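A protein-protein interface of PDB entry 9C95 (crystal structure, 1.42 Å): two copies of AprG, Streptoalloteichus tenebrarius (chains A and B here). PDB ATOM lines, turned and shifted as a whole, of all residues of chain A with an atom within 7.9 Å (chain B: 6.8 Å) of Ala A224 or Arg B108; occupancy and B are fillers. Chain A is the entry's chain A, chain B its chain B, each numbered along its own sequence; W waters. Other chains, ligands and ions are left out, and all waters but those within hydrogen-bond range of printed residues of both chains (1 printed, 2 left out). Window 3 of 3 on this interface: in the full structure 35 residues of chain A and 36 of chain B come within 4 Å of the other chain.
The backbone carbonyl oxygen of Ala B98 is in hydrogen-bond range of the backbone NH of Arg B103, 2.9 Å away. The side-chain hydroxyl (OG) of Ser B107 lies within hydrogen-bond range of a ring nitrogen (ND1) of His B99, 3.2 Å away. The side-chain hydroxyl (OG) of Ser B107 lies within hydrogen-bond range of the backbone carbonyl oxygen (O) of Phe B104 (3.4 Å). O of Arg B108 is in hydrogen-bond range of OG of Ser B112, at 2.9 Å.
The backbone NH (N) of Gly B105 sits close to the backbone carbonyl oxygen (O) of Glu A223. O of Ala A224 is in hydrogen-bond range of NE of Arg B108 (2.9 Å). OE2 of Glu A226 lies within salt-bridge range of NZ of Lys B109.
Of the 17 printed residues of chain A, 4 touch a printed residue of chain B. Of the 18 printed residues of chain B, 7 touch a printed residue of chain A. Hydrophobic or aromatic side chains of chain B that line the printed part of chain A: His B99 and Phe B104. Among the printed residues, 9 pairs touch across the chains. Among the printed residues, Asp or Glu carboxylates within 4 Å of a Lys or Arg side-chain nitrogen of the other chain: Glu A226 with Lys B109 (2.6 Å).
Water W1 bridges the backbone carbonyl oxygen of Gly B102 (2.7 Å) and the side-chain carboxylate of Glu A223 (2.8 Å).
Of the printed residues of chain B, Leu A151 touches His B99 and Phe B104. Of the printed residues of chain B, Ala A224 touches Phe B104, Gly B105 and Arg B108. Printed residues of chain A within 4 Å of His B99: Leu A151. No residue of chain A comes within 4 Å of Ser B107. The nearest printed residue of chain B that does not touch Ala A224 is Arg B103 (6.4 Å). The nearest printed residue of chain A that does not touch Lys B109 is Glu A223 (6.1 Å).
No position is printed for both chains. Of the 9 pairs that touch across the chains among the printed residues, none has its exchanged pair printed and touching as well.
O of Leu A151 touches CE1 of His B99, 3.9 Å away. Leu A151 touches Phe B104. Glu A223 touches Gly B102. Glu A223 touches Arg B103. Ala A224 touches Phe B104. Ala A224 touches Gly B105.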
ATOM      1  N   LEU A 151     -10.854  26.723  -0.638  1.00  0.00           N
ATOM      2  CA  LEU A 151      -9.495  26.194  -0.564  1.00  0.00           C
ATOM      3  C   LEU A 151      -9.433  24.723  -0.971  1.00  0.00           C
ATOM      4  O   LEU A 151      -8.585  24.326  -1.782  1.00  0.00           O
ATOM      5  CB  LEU A 151      -8.963  26.408   0.859  1.00  0.00           C
ATOM      6  CG  LEU A 151      -7.564  26.902   1.117  1.00  0.00           C
ATOM      7  CD1 LEU A 151      -7.081  27.958   0.137  1.00  0.00           C
ATOM      8  CD2 LEU A 151      -7.486  27.402   2.606  1.00  0.00           C
ATOM      9  N   VAL A 156      -8.764  29.462  -5.096  1.00  0.00           N
ATOM     10  CA  VAL A 156      -7.995  30.184  -4.096  1.00  0.00           C
ATOM     11  C   VAL A 156      -8.335  31.666  -4.102  1.00  0.00           C
ATOM     12  O   VAL A 156      -8.320  32.308  -3.055  1.00  0.00           O
ATOM     13  CB  VAL A 156      -6.488  29.931  -4.269  1.00  0.00           C
ATOM     14  CG1 VAL A 156      -5.674  30.696  -3.192  1.00  0.00           C
ATOM     15  CG2 VAL A 156      -6.190  28.440  -4.167  1.00  0.00           C
ATOM     16  N   ALA A 159     -11.149  32.190  -1.859  1.00  0.00           N
ATOM     17  CA  ALA A 159     -10.687  32.134  -0.466  1.00  0.00           C
ATOM     18  C   ALA A 159      -9.999  33.431  -0.038  1.00  0.00           C
ATOM     19  O   ALA A 159     -10.216  33.925   1.079  1.00  0.00           O
ATOM     20  CB  ALA A 159      -9.760  30.930  -0.247  1.00  0.00           C
ATOM     21  N   ARG A 160      -9.138  33.991  -0.902  1.00  0.00           N
ATOM     22  CA  ARG A 160      -8.472  35.241  -0.548  1.00  0.00           C
ATOM     23  C   ARG A 160      -9.488  36.355  -0.335  1.00  0.00           C
ATOM     24  O   ARG A 160      -9.347  37.163   0.588  1.00  0.00           O
ATOM     25  CB  ARG A 160      -7.486  35.624  -1.660  1.00  0.00           C
ATOM     26  CG  ARG A 160      -6.248  34.749  -1.744  1.00  0.00           C
ATOM     27  CD  ARG A 160      -5.337  35.354  -2.819  1.00  0.00           C
ATOM     28  NE  ARG A 160      -4.070  34.653  -3.010  1.00  0.00           N
ATOM     29  CZ  ARG A 160      -2.958  34.987  -2.341  1.00  0.00           C
ATOM     30  NH1 ARG A 160      -2.989  35.956  -1.445  1.00  0.00           N
ATOM     31  NH2 ARG A 160      -1.818  34.360  -2.591  1.00  0.00           N
ATOM     32  N   PHE A 217      -9.756  28.898   9.310  1.00  0.00           N
ATOM     33  CA  PHE A 217      -9.706  29.114   7.868  1.00  0.00           C
ATOM     34  C   PHE A 217      -8.510  29.979   7.483  1.00  0.00           C
ATOM     35  O   PHE A 217      -7.793  29.676   6.522  1.00  0.00           O
ATOM     36  CB  PHE A 217     -11.006  29.794   7.420  1.00  0.00           C
ATOM     37  CG  PHE A 217     -10.871  30.492   6.107  1.00  0.00           C
ATOM     38  CD1 PHE A 217     -10.530  29.779   4.974  1.00  0.00           C
ATOM     39  CD2 PHE A 217     -11.022  31.875   6.022  1.00  0.00           C
ATOM     40  CE1 PHE A 217     -10.332  30.412   3.774  1.00  0.00           C
ATOM     41  CE2 PHE A 217     -10.864  32.534   4.776  1.00  0.00           C
ATOM     42  CZ  PHE A 217     -10.513  31.786   3.652  1.00  0.00           C
ATOM     43  N   LEU A 218      -8.263  31.055   8.220  1.00  0.00           N
ATOM     44  CA  LEU A 218      -7.156  31.925   7.843  1.00  0.00           C
ATOM     45  C   LEU A 218      -5.811  31.216   7.952  1.00  0.00           C
ATOM     46  O   LEU A 218      -4.898  31.488   7.151  1.00  0.00           O
ATOM     47  CB  LEU A 218      -7.193  33.161   8.732  1.00  0.00           C
ATOM     48  CG  LEU A 218      -8.335  34.126   8.409  1.00  0.00           C
ATOM     49  CD1 LEU A 218      -8.612  35.061   9.613  1.00  0.00           C
ATOM     50  CD2 LEU A 218      -8.041  34.936   7.161  1.00  0.00           C
ATOM     51  N   THR A 219      -5.660  30.334   8.962  1.00  0.00           N
ATOM     52  CA  THR A 219      -4.422  29.582   9.070  1.00  0.00           C
ATOM     53  C   THR A 219      -4.250  28.640   7.895  1.00  0.00           C
ATOM     54  O   THR A 219      -3.159  28.535   7.343  1.00  0.00           O
ATOM     55  CB  THR A 219      -4.403  28.835  10.403  1.00  0.00           C
ATOM     56  OG1 THR A 219      -4.582  29.760  11.490  1.00  0.00           O
ATOM     57  CG2 THR A 219      -3.052  28.130  10.585  1.00  0.00           C
ATOM     58  N   ALA A 220      -5.332  27.975   7.465  1.00  0.00           N
ATOM     59  CA  ALA A 220      -5.253  27.113   6.292  1.00  0.00           C
ATOM     60  C   ALA A 220      -4.912  27.910   5.036  1.00  0.00           C
ATOM     61  O   ALA A 220      -4.158  27.441   4.176  1.00  0.00           O
ATOM     62  CB  ALA A 220      -6.581  26.357   6.102  1.00  0.00           C
ATOM     63  N   LEU A 221      -5.491  29.112   4.898  1.00  0.00           N
ATOM     64  CA  LEU A 221      -5.182  29.978   3.770  1.00  0.00           C
ATOM     65  C   LEU A 221      -3.719  30.428   3.776  1.00  0.00           C
ATOM     66  O   LEU A 221      -3.071  30.433   2.715  1.00  0.00           O
ATOM     67  CB  LEU A 221      -6.155  31.152   3.741  1.00  0.00           C
ATOM     68  CG  LEU A 221      -5.939  32.136   2.586  1.00  0.00           C
ATOM     69  CD1 LEU A 221      -6.118  31.493   1.248  1.00  0.00           C
ATOM     70  CD2 LEU A 221      -6.864  33.354   2.737  1.00  0.00           C
ATOM     71  N   TYR A 222      -3.169  30.724   4.963  1.00  0.00           N
ATOM     72  CA  TYR A 222      -1.733  30.961   5.061  1.00  0.00           C
ATOM     73  C   TYR A 222      -0.934  29.732   4.638  1.00  0.00           C
ATOM     74  O   TYR A 222       0.054  29.847   3.891  1.00  0.00           O
ATOM     75  CB  TYR A 222      -1.378  31.368   6.490  1.00  0.00           C
ATOM     76  CG  TYR A 222       0.125  31.428   6.669  1.00  0.00           C
ATOM     77  CD1 TYR A 222       0.875  32.434   6.043  1.00  0.00           C
ATOM     78  CD2 TYR A 222       0.785  30.480   7.439  1.00  0.00           C
ATOM     79  CE1 TYR A 222       2.265  32.481   6.196  1.00  0.00           C
ATOM     80  CE2 TYR A 222       2.171  30.500   7.589  1.00  0.00           C
ATOM     81  CZ  TYR A 222       2.888  31.513   6.960  1.00  0.00           C
ATOM     82  OH  TYR A 222       4.254  31.565   7.117  1.00  0.00           O
ATOM     83  N   GLU A 223      -1.323  28.542   5.096  1.00  0.00           N
ATOM     84  CA  GLU A 223      -0.600  27.351   4.660  1.00  0.00           C
ATOM     85  C   GLU A 223      -0.609  27.235   3.136  1.00  0.00           C
ATOM     86  O   GLU A 223       0.418  26.908   2.526  1.00  0.00           O
ATOM     87  CB  GLU A 223      -1.193  26.089   5.305  1.00  0.00           C
ATOM     88  CG  GLU A 223      -0.492  24.841   4.817  1.00  0.00           C
ATOM     89  CD  GLU A 223      -0.739  23.626   5.686  1.00  0.00           C
ATOM     90  OE1 GLU A 223       0.009  22.626   5.556  1.00  0.00           O
ATOM     91  OE2 GLU A 223      -1.649  23.690   6.515  1.00  0.00           O
ATOM     92  N   ALA A 224      -1.744  27.564   2.499  1.00  0.00           N
ATOM     93  CA  ALA A 224      -1.889  27.432   1.050  1.00  0.00           C
ATOM     94  C   ALA A 224      -1.078  28.465   0.274  1.00  0.00           C
ATOM     95  O   ALA A 224      -0.637  28.176  -0.844  1.00  0.00           O
ATOM     96  CB  ALA A 224      -3.369  27.561   0.664  1.00  0.00           C
ATOM     97  N   THR A 225      -0.919  29.677   0.813  1.00  0.00           N
ATOM     98  CA  THR A 225      -0.395  30.812   0.052  1.00  0.00           C
ATOM     99  C   THR A 225       0.924  31.358   0.567  1.00  0.00           C
ATOM    100  O   THR A 225       1.642  32.018  -0.211  1.00  0.00           O
ATOM    101  CB  THR A 225      -1.379  31.994   0.076  1.00  0.00           C
ATOM    102  OG1 THR A 225      -1.563  32.444   1.437  1.00  0.00           O
ATOM    103  CG2 THR A 225      -2.696  31.652  -0.581  1.00  0.00           C
ATOM    104  N   GLU A 226       1.247  31.143   1.842  1.00  0.00           N
ATOM    105  CA  GLU A 226       2.391  31.745   2.528  1.00  0.00           C
ATOM    106  C   GLU A 226       2.323  33.253   2.569  1.00  0.00           C
ATOM    107  O   GLU A 226       3.350  33.909   2.770  1.00  0.00           O
ATOM    108  CB  GLU A 226       3.735  31.241   2.004  1.00  0.00           C
ATOM    109  CG  GLU A 226       4.113  29.942   2.673  1.00  0.00           C
ATOM    110  CD  GLU A 226       5.118  29.162   1.869  1.00  0.00           C
ATOM    111  OE1 GLU A 226       6.062  29.771   1.320  1.00  0.00           O
ATOM    112  OE2 GLU A 226       4.955  27.939   1.769  1.00  0.00           O
ATOM    113  N   ASP A 227       1.126  33.815   2.432  1.00  0.00           N
ATOM    114  CA  ASP A 227       0.928  35.259   2.551  1.00  0.00           C
ATOM    115  C   ASP A 227       0.763  35.597   4.029  1.00  0.00           C
ATOM    116  O   ASP A 227      -0.245  35.249   4.649  1.00  0.00           O
ATOM    117  CB  ASP A 227      -0.293  35.675   1.734  1.00  0.00           C
ATOM    118  CG  ASP A 227      -0.493  37.169   1.690  1.00  0.00           C
ATOM    119  OD1 ASP A 227      -0.060  37.877   2.634  1.00  0.00           O
ATOM    120  OD2 ASP A 227      -1.101  37.633   0.703  1.00  0.00           O
ATOM    121  N   TYR A 230      -2.445  36.701   6.178  1.00  0.00           N
ATOM    122  CA  TYR A 230      -3.429  35.776   6.701  1.00  0.00           C
ATOM    123  C   TYR A 230      -2.977  35.158   8.012  1.00  0.00           C
ATOM    124  O   TYR A 230      -3.798  34.956   8.925  1.00  0.00           O
ATOM    125  CB  TYR A 230      -3.734  34.695   5.646  1.00  0.00           C
ATOM    126  CG  TYR A 230      -4.094  35.252   4.284  1.00  0.00           C
ATOM    127  CD1 TYR A 230      -4.991  36.321   4.159  1.00  0.00           C
ATOM    128  CD2 TYR A 230      -3.549  34.699   3.139  1.00  0.00           C
ATOM    129  CE1 TYR A 230      -5.302  36.846   2.910  1.00  0.00           C
ATOM    130  CE2 TYR A 230      -3.854  35.198   1.896  1.00  0.00           C
ATOM    131  CZ  TYR A 230      -4.721  36.274   1.789  1.00  0.00           C
ATOM    132  OH  TYR A 230      -5.015  36.742   0.537  1.00  0.00           O
ATOM    133  N   LEU A 268       2.576  24.911  12.121  1.00  0.00           N
ATOM    134  CA  LEU A 268       3.206  25.858  11.196  1.00  0.00           C
ATOM    135  C   LEU A 268       4.240  26.769  11.872  1.00  0.00           C
ATOM    136  O   LEU A 268       5.189  27.175  11.203  1.00  0.00           O
ATOM    137  CB  LEU A 268       2.147  26.711  10.508  1.00  0.00           C
ATOM    138  CG  LEU A 268       1.121  25.887   9.723  1.00  0.00           C
ATOM    139  CD1 LEU A 268       0.147  26.847   9.079  1.00  0.00           C
ATOM    140  CD2 LEU A 268       1.763  25.037   8.653  1.00  0.00           C
ATOM    141  N   THR B  95       0.910  14.678  -4.799  1.00  0.00           N
ATOM    142  CA  THR B  95       0.042  15.849  -4.863  1.00  0.00           C
ATOM    143  C   THR B  95      -1.342  15.531  -4.318  1.00  0.00           C
ATOM    144  O   THR B  95      -1.888  16.300  -3.521  1.00  0.00           O
ATOM    145  CB  THR B  95      -0.069  16.332  -6.313  1.00  0.00           C
ATOM    146  OG1 THR B  95       1.230  16.719  -6.816  1.00  0.00           O
ATOM    147  CG2 THR B  95      -1.014  17.524  -6.410  1.00  0.00           C
ATOM    148  N   ALA B  98      -1.251  14.905  -0.450  1.00  0.00           N
ATOM    149  CA  ALA B  98      -1.030  16.148   0.278  1.00  0.00           C
ATOM    150  C   ALA B  98      -2.281  16.998   0.289  1.00  0.00           C
ATOM    151  O   ALA B  98      -2.651  17.570   1.322  1.00  0.00           O
ATOM    152  CB  ALA B  98       0.105  16.952  -0.382  1.00  0.00           C
ATOM    153  N   HIS B  99      -2.965  17.083  -0.861  1.00  0.00           N
ATOM    154  CA  HIS B  99      -4.143  17.946  -0.932  1.00  0.00           C
ATOM    155  C   HIS B  99      -5.265  17.441  -0.049  1.00  0.00           C
ATOM    156  O   HIS B  99      -5.897  18.229   0.672  1.00  0.00           O
ATOM    157  CB  HIS B  99      -4.617  18.095  -2.379  1.00  0.00           C
ATOM    158  CG  HIS B  99      -5.624  19.192  -2.542  1.00  0.00           C
ATOM    159  ND1 HIS B  99      -5.247  20.511  -2.658  1.00  0.00           N
ATOM    160  CD2 HIS B  99      -6.979  19.178  -2.537  1.00  0.00           C
ATOM    161  CE1 HIS B  99      -6.330  21.264  -2.777  1.00  0.00           C
ATOM    162  NE2 HIS B  99      -7.393  20.482  -2.694  1.00  0.00           N
ATOM    163  N   GLY B 102      -5.165  18.344   3.407  1.00  0.00           N
ATOM    164  CA  GLY B 102      -5.173  19.740   3.753  1.00  0.00           C
ATOM    165  C   GLY B 102      -3.804  20.380   3.801  1.00  0.00           C
ATOM    166  O   GLY B 102      -3.682  21.512   4.301  1.00  0.00           O
ATOM    167  N   ARG B 103      -2.760  19.684   3.322  1.00  0.00           N
ATOM    168  CA  ARG B 103      -1.408  20.258   3.270  1.00  0.00           C
ATOM    169  C   ARG B 103      -1.303  21.083   1.986  1.00  0.00           C
ATOM    170  O   ARG B 103      -0.677  20.685   1.002  1.00  0.00           O
ATOM    171  CB  ARG B 103      -0.342  19.164   3.305  1.00  0.00           C
ATOM    172  CG  ARG B 103      -0.293  18.335   4.616  1.00  0.00           C
ATOM    173  CD  ARG B 103       0.468  19.070   5.659  1.00  0.00           C
ATOM    174  NE  ARG B 103       0.699  18.257   6.863  1.00  0.00           N
ATOM    175  CZ  ARG B 103       1.903  17.832   7.267  1.00  0.00           C
ATOM    176  NH1 ARG B 103       3.012  18.130   6.585  1.00  0.00           N
ATOM    177  NH2 ARG B 103       1.978  17.111   8.385  1.00  0.00           N
ATOM    178  N   PHE B 104      -1.946  22.256   2.011  1.00  0.00           N
ATOM    179  CA  PHE B 104      -2.176  23.024   0.786  1.00  0.00           C
ATOM    180  C   PHE B 104      -0.918  23.662   0.238  1.00  0.00           C
ATOM    181  O   PHE B 104      -0.843  23.915  -0.964  1.00  0.00           O
ATOM    182  CB  PHE B 104      -3.228  24.093   1.024  1.00  0.00           C
ATOM    183  CG  PHE B 104      -4.611  23.537   1.326  1.00  0.00           C
ATOM    184  CD1 PHE B 104      -5.187  22.535   0.538  1.00  0.00           C
ATOM    185  CD2 PHE B 104      -5.320  24.027   2.404  1.00  0.00           C
ATOM    186  CE1 PHE B 104      -6.485  22.019   0.830  1.00  0.00           C
ATOM    187  CE2 PHE B 104      -6.622  23.546   2.698  1.00  0.00           C
ATOM    188  CZ  PHE B 104      -7.195  22.545   1.933  1.00  0.00           C
ATOM    189  N   GLY B 105       0.062  23.944   1.091  1.00  0.00           N
ATOM    190  CA  GLY B 105       1.309  24.479   0.576  1.00  0.00           C
ATOM    191  C   GLY B 105       2.085  23.399  -0.138  1.00  0.00           C
ATOM    192  O   GLY B 105       2.634  23.632  -1.230  1.00  0.00           O
ATOM    193  N   LEU B 106       2.098  22.195   0.440  1.00  0.00           N
ATOM    194  CA  LEU B 106       2.751  21.059  -0.209  1.00  0.00           C
ATOM    195  C   LEU B 106       2.069  20.726  -1.528  1.00  0.00           C
ATOM    196  O   LEU B 106       2.727  20.562  -2.557  1.00  0.00           O
ATOM    197  CB  LEU B 106       2.755  19.858   0.736  1.00  0.00           C
ATOM    198  CG  LEU B 106       3.406  18.552   0.246  1.00  0.00           C
ATOM    199  CD1 LEU B 106       4.884  18.765  -0.133  1.00  0.00           C
ATOM    200  CD2 LEU B 106       3.302  17.464   1.319  1.00  0.00           C
ATOM    201  N   SER B 107       0.732  20.662  -1.536  1.00  0.00           N
ATOM    202  CA  SER B 107       0.059  20.316  -2.776  1.00  0.00           C
ATOM    203  C   SER B 107       0.243  21.396  -3.842  1.00  0.00           C
ATOM    204  O   SER B 107       0.446  21.067  -5.009  1.00  0.00           O
ATOM    205  CB  SER B 107      -1.408  19.935  -2.528  1.00  0.00           C
ATOM    206  OG  SER B 107      -2.171  21.073  -2.215  1.00  0.00           O
ATOM    207  N   ARG B 108       0.197  22.679  -3.456  1.00  0.00           N
ATOM    208  CA  ARG B 108       0.427  23.738  -4.447  1.00  0.00           C
ATOM    209  C   ARG B 108       1.829  23.645  -5.046  1.00  0.00           C
ATOM    210  O   ARG B 108       1.994  23.748  -6.269  1.00  0.00           O
ATOM    211  CB  ARG B 108       0.196  25.117  -3.833  1.00  0.00           C
ATOM    212  CG  ARG B 108       0.613  26.254  -4.798  1.00  0.00           C
ATOM    213  CD  ARG B 108       0.420  27.627  -4.190  1.00  0.00           C
ATOM    214  NE  ARG B 108       1.254  27.824  -3.018  1.00  0.00           N
ATOM    215  CZ  ARG B 108       2.543  28.141  -3.052  1.00  0.00           C
ATOM    216  NH1 ARG B 108       3.154  28.309  -4.215  1.00  0.00           N
ATOM    217  NH2 ARG B 108       3.214  28.323  -1.928  1.00  0.00           N
ATOM    218  N   LYS B 109       2.839  23.406  -4.209  1.00  0.00           N
ATOM    219  CA  LYS B 109       4.207  23.378  -4.727  1.00  0.00           C
ATOM    220  C   LYS B 109       4.424  22.154  -5.598  1.00  0.00           C
ATOM    221  O   LYS B 109       5.003  22.261  -6.680  1.00  0.00           O
ATOM    222  CB  LYS B 109       5.197  23.421  -3.575  1.00  0.00           C
ATOM    223  CG  LYS B 109       5.175  24.791  -2.880  1.00  0.00           C
ATOM    224  CD  LYS B 109       5.871  24.713  -1.540  1.00  0.00           C
ATOM    225  CE  LYS B 109       5.714  26.043  -0.788  1.00  0.00           C
ATOM    226  NZ  LYS B 109       6.149  25.897   0.625  1.00  0.00           N
ATOM    227  N   LEU B 110       3.918  20.993  -5.164  1.00  0.00           N
ATOM    228  CA  LEU B 110       4.059  19.796  -5.981  1.00  0.00           C
ATOM    229  C   LEU B 110       3.332  19.922  -7.315  1.00  0.00           C
ATOM    230  O   LEU B 110       3.860  19.531  -8.360  1.00  0.00           O
ATOM    231  CB  LEU B 110       3.505  18.589  -5.222  1.00  0.00           C
ATOM    232  CG  LEU B 110       4.267  18.105  -4.016  1.00  0.00           C
ATOM    233  CD1 LEU B 110       3.379  17.082  -3.244  1.00  0.00           C
ATOM    234  CD2 LEU B 110       5.577  17.509  -4.470  1.00  0.00           C
ATOM    235  N   MET B 111       2.111  20.455  -7.299  1.00  0.00           N
ATOM    236  CA  MET B 111       1.325  20.515  -8.521  1.00  0.00           C
ATOM    237  C   MET B 111       1.905  21.543  -9.479  1.00  0.00           C
ATOM    238  O   MET B 111       1.856  21.365 -10.705  1.00  0.00           O
ATOM    239  CB  MET B 111      -0.130  20.883  -8.196  1.00  0.00           C
ATOM    240  CG  MET B 111      -1.029  20.839  -9.449  1.00  0.00           C
ATOM    241  SD  MET B 111      -1.319  19.143  -9.977  1.00  0.00           S
ATOM    242  CE  MET B 111      -1.383  19.337 -11.768  1.00  0.00           C
ATOM    243  N   SER B 112       2.428  22.635  -8.931  1.00  0.00           N
ATOM    244  CA  SER B 112       3.058  23.638  -9.791  1.00  0.00           C
ATOM    245  C   SER B 112       4.280  23.066 -10.487  1.00  0.00           C
ATOM    246  O   SER B 112       4.498  23.325 -11.676  1.00  0.00           O
ATOM    247  CB  SER B 112       3.381  24.889  -8.986  1.00  0.00           C
ATOM    248  OG  SER B 112       2.144  25.510  -8.594  1.00  0.00           O
ATOM    249  N   PHE B 113       5.056  22.230  -9.807  1.00  0.00           N
ATOM    250  CA  PHE B 113       6.155  21.575 -10.524  1.00  0.00           C
ATOM    251  C   PHE B 113       5.627  20.646 -11.621  1.00  0.00           C
ATOM    252  O   PHE B 113       6.121  20.644 -12.758  1.00  0.00           O
ATOM    253  CB  PHE B 113       7.089  20.823  -9.574  1.00  0.00           C
ATOM    254  CG  PHE B 113       8.077  19.989 -10.328  1.00  0.00           C
ATOM    255  CD1 PHE B 113       9.213  20.589 -10.897  1.00  0.00           C
ATOM    256  CD2 PHE B 113       7.812  18.652 -10.619  1.00  0.00           C
ATOM    257  CE1 PHE B 113      10.093  19.840 -11.677  1.00  0.00           C
ATOM    258  CE2 PHE B 113       8.688  17.892 -11.387  1.00  0.00           C
ATOM    259  CZ  PHE B 113       9.848  18.488 -11.921  1.00  0.00           C
ATOM    260  N   GLU B 115       2.990  20.887 -13.382  1.00  0.00           N
ATOM    261  CA  GLU B 115       2.597  21.706 -14.536  1.00  0.00           C
ATOM    262  C   GLU B 115       3.771  22.238 -15.361  1.00  0.00           C
ATOM    263  O   GLU B 115       3.581  22.518 -16.555  1.00  0.00           O
ATOM    264  CB  GLU B 115       1.673  22.832 -14.085  1.00  0.00           C
ATOM    265  CG  GLU B 115       0.409  22.197 -13.522  1.00  0.00           C
ATOM    266  CD  GLU B 115      -0.712  23.164 -13.209  1.00  0.00           C
ATOM    267  OE1 GLU B 115      -1.809  22.990 -13.787  1.00  0.00           O
ATOM    268  OE2 GLU B 115      -0.513  24.073 -12.359  1.00  0.00           O
ATOM    269  N   THR B 153      -6.809  19.057  -7.097  1.00  0.00           N
ATOM    270  CA  THR B 153      -6.400  20.401  -6.704  1.00  0.00           C
ATOM    271  C   THR B 153      -7.239  21.489  -7.367  1.00  0.00           C
ATOM    272  O   THR B 153      -6.948  22.666  -7.168  1.00  0.00           O
ATOM    273  CB  THR B 153      -4.903  20.649  -6.975  1.00  0.00           C
ATOM    274  OG1 THR B 153      -4.641  20.473  -8.384  1.00  0.00           O
ATOM    275  CG2 THR B 153      -4.034  19.697  -6.170  1.00  0.00           C
ATOM    276  N   ARG B 155      -7.542  22.217 -10.561  1.00  0.00           N
ATOM    277  CA  ARG B 155      -6.983  22.744 -11.812  1.00  0.00           C
ATOM    278  C   ARG B 155      -7.664  22.038 -12.985  1.00  0.00           C
ATOM    279  O   ARG B 155      -7.074  21.252 -13.703  1.00  0.00           O
ATOM    280  CB  ARG B 155      -5.463  22.603 -11.826  1.00  0.00           C
ATOM    281  CG  ARG B 155      -4.824  23.538 -10.828  1.00  0.00           C
ATOM    282  CD  ARG B 155      -3.330  23.412 -10.656  1.00  0.00           C
ATOM    283  NE  ARG B 155      -3.057  23.666  -9.239  1.00  0.00           N
ATOM    284  CZ  ARG B 155      -1.956  24.198  -8.718  1.00  0.00           C
ATOM    285  NH1 ARG B 155      -1.904  24.345  -7.392  1.00  0.00           N
ATOM    286  NH2 ARG B 155      -0.924  24.569  -9.480  1.00  0.00           N
HETATM  287  O   HOH W   1      -4.349  23.572   5.929  1.00  0.00           O
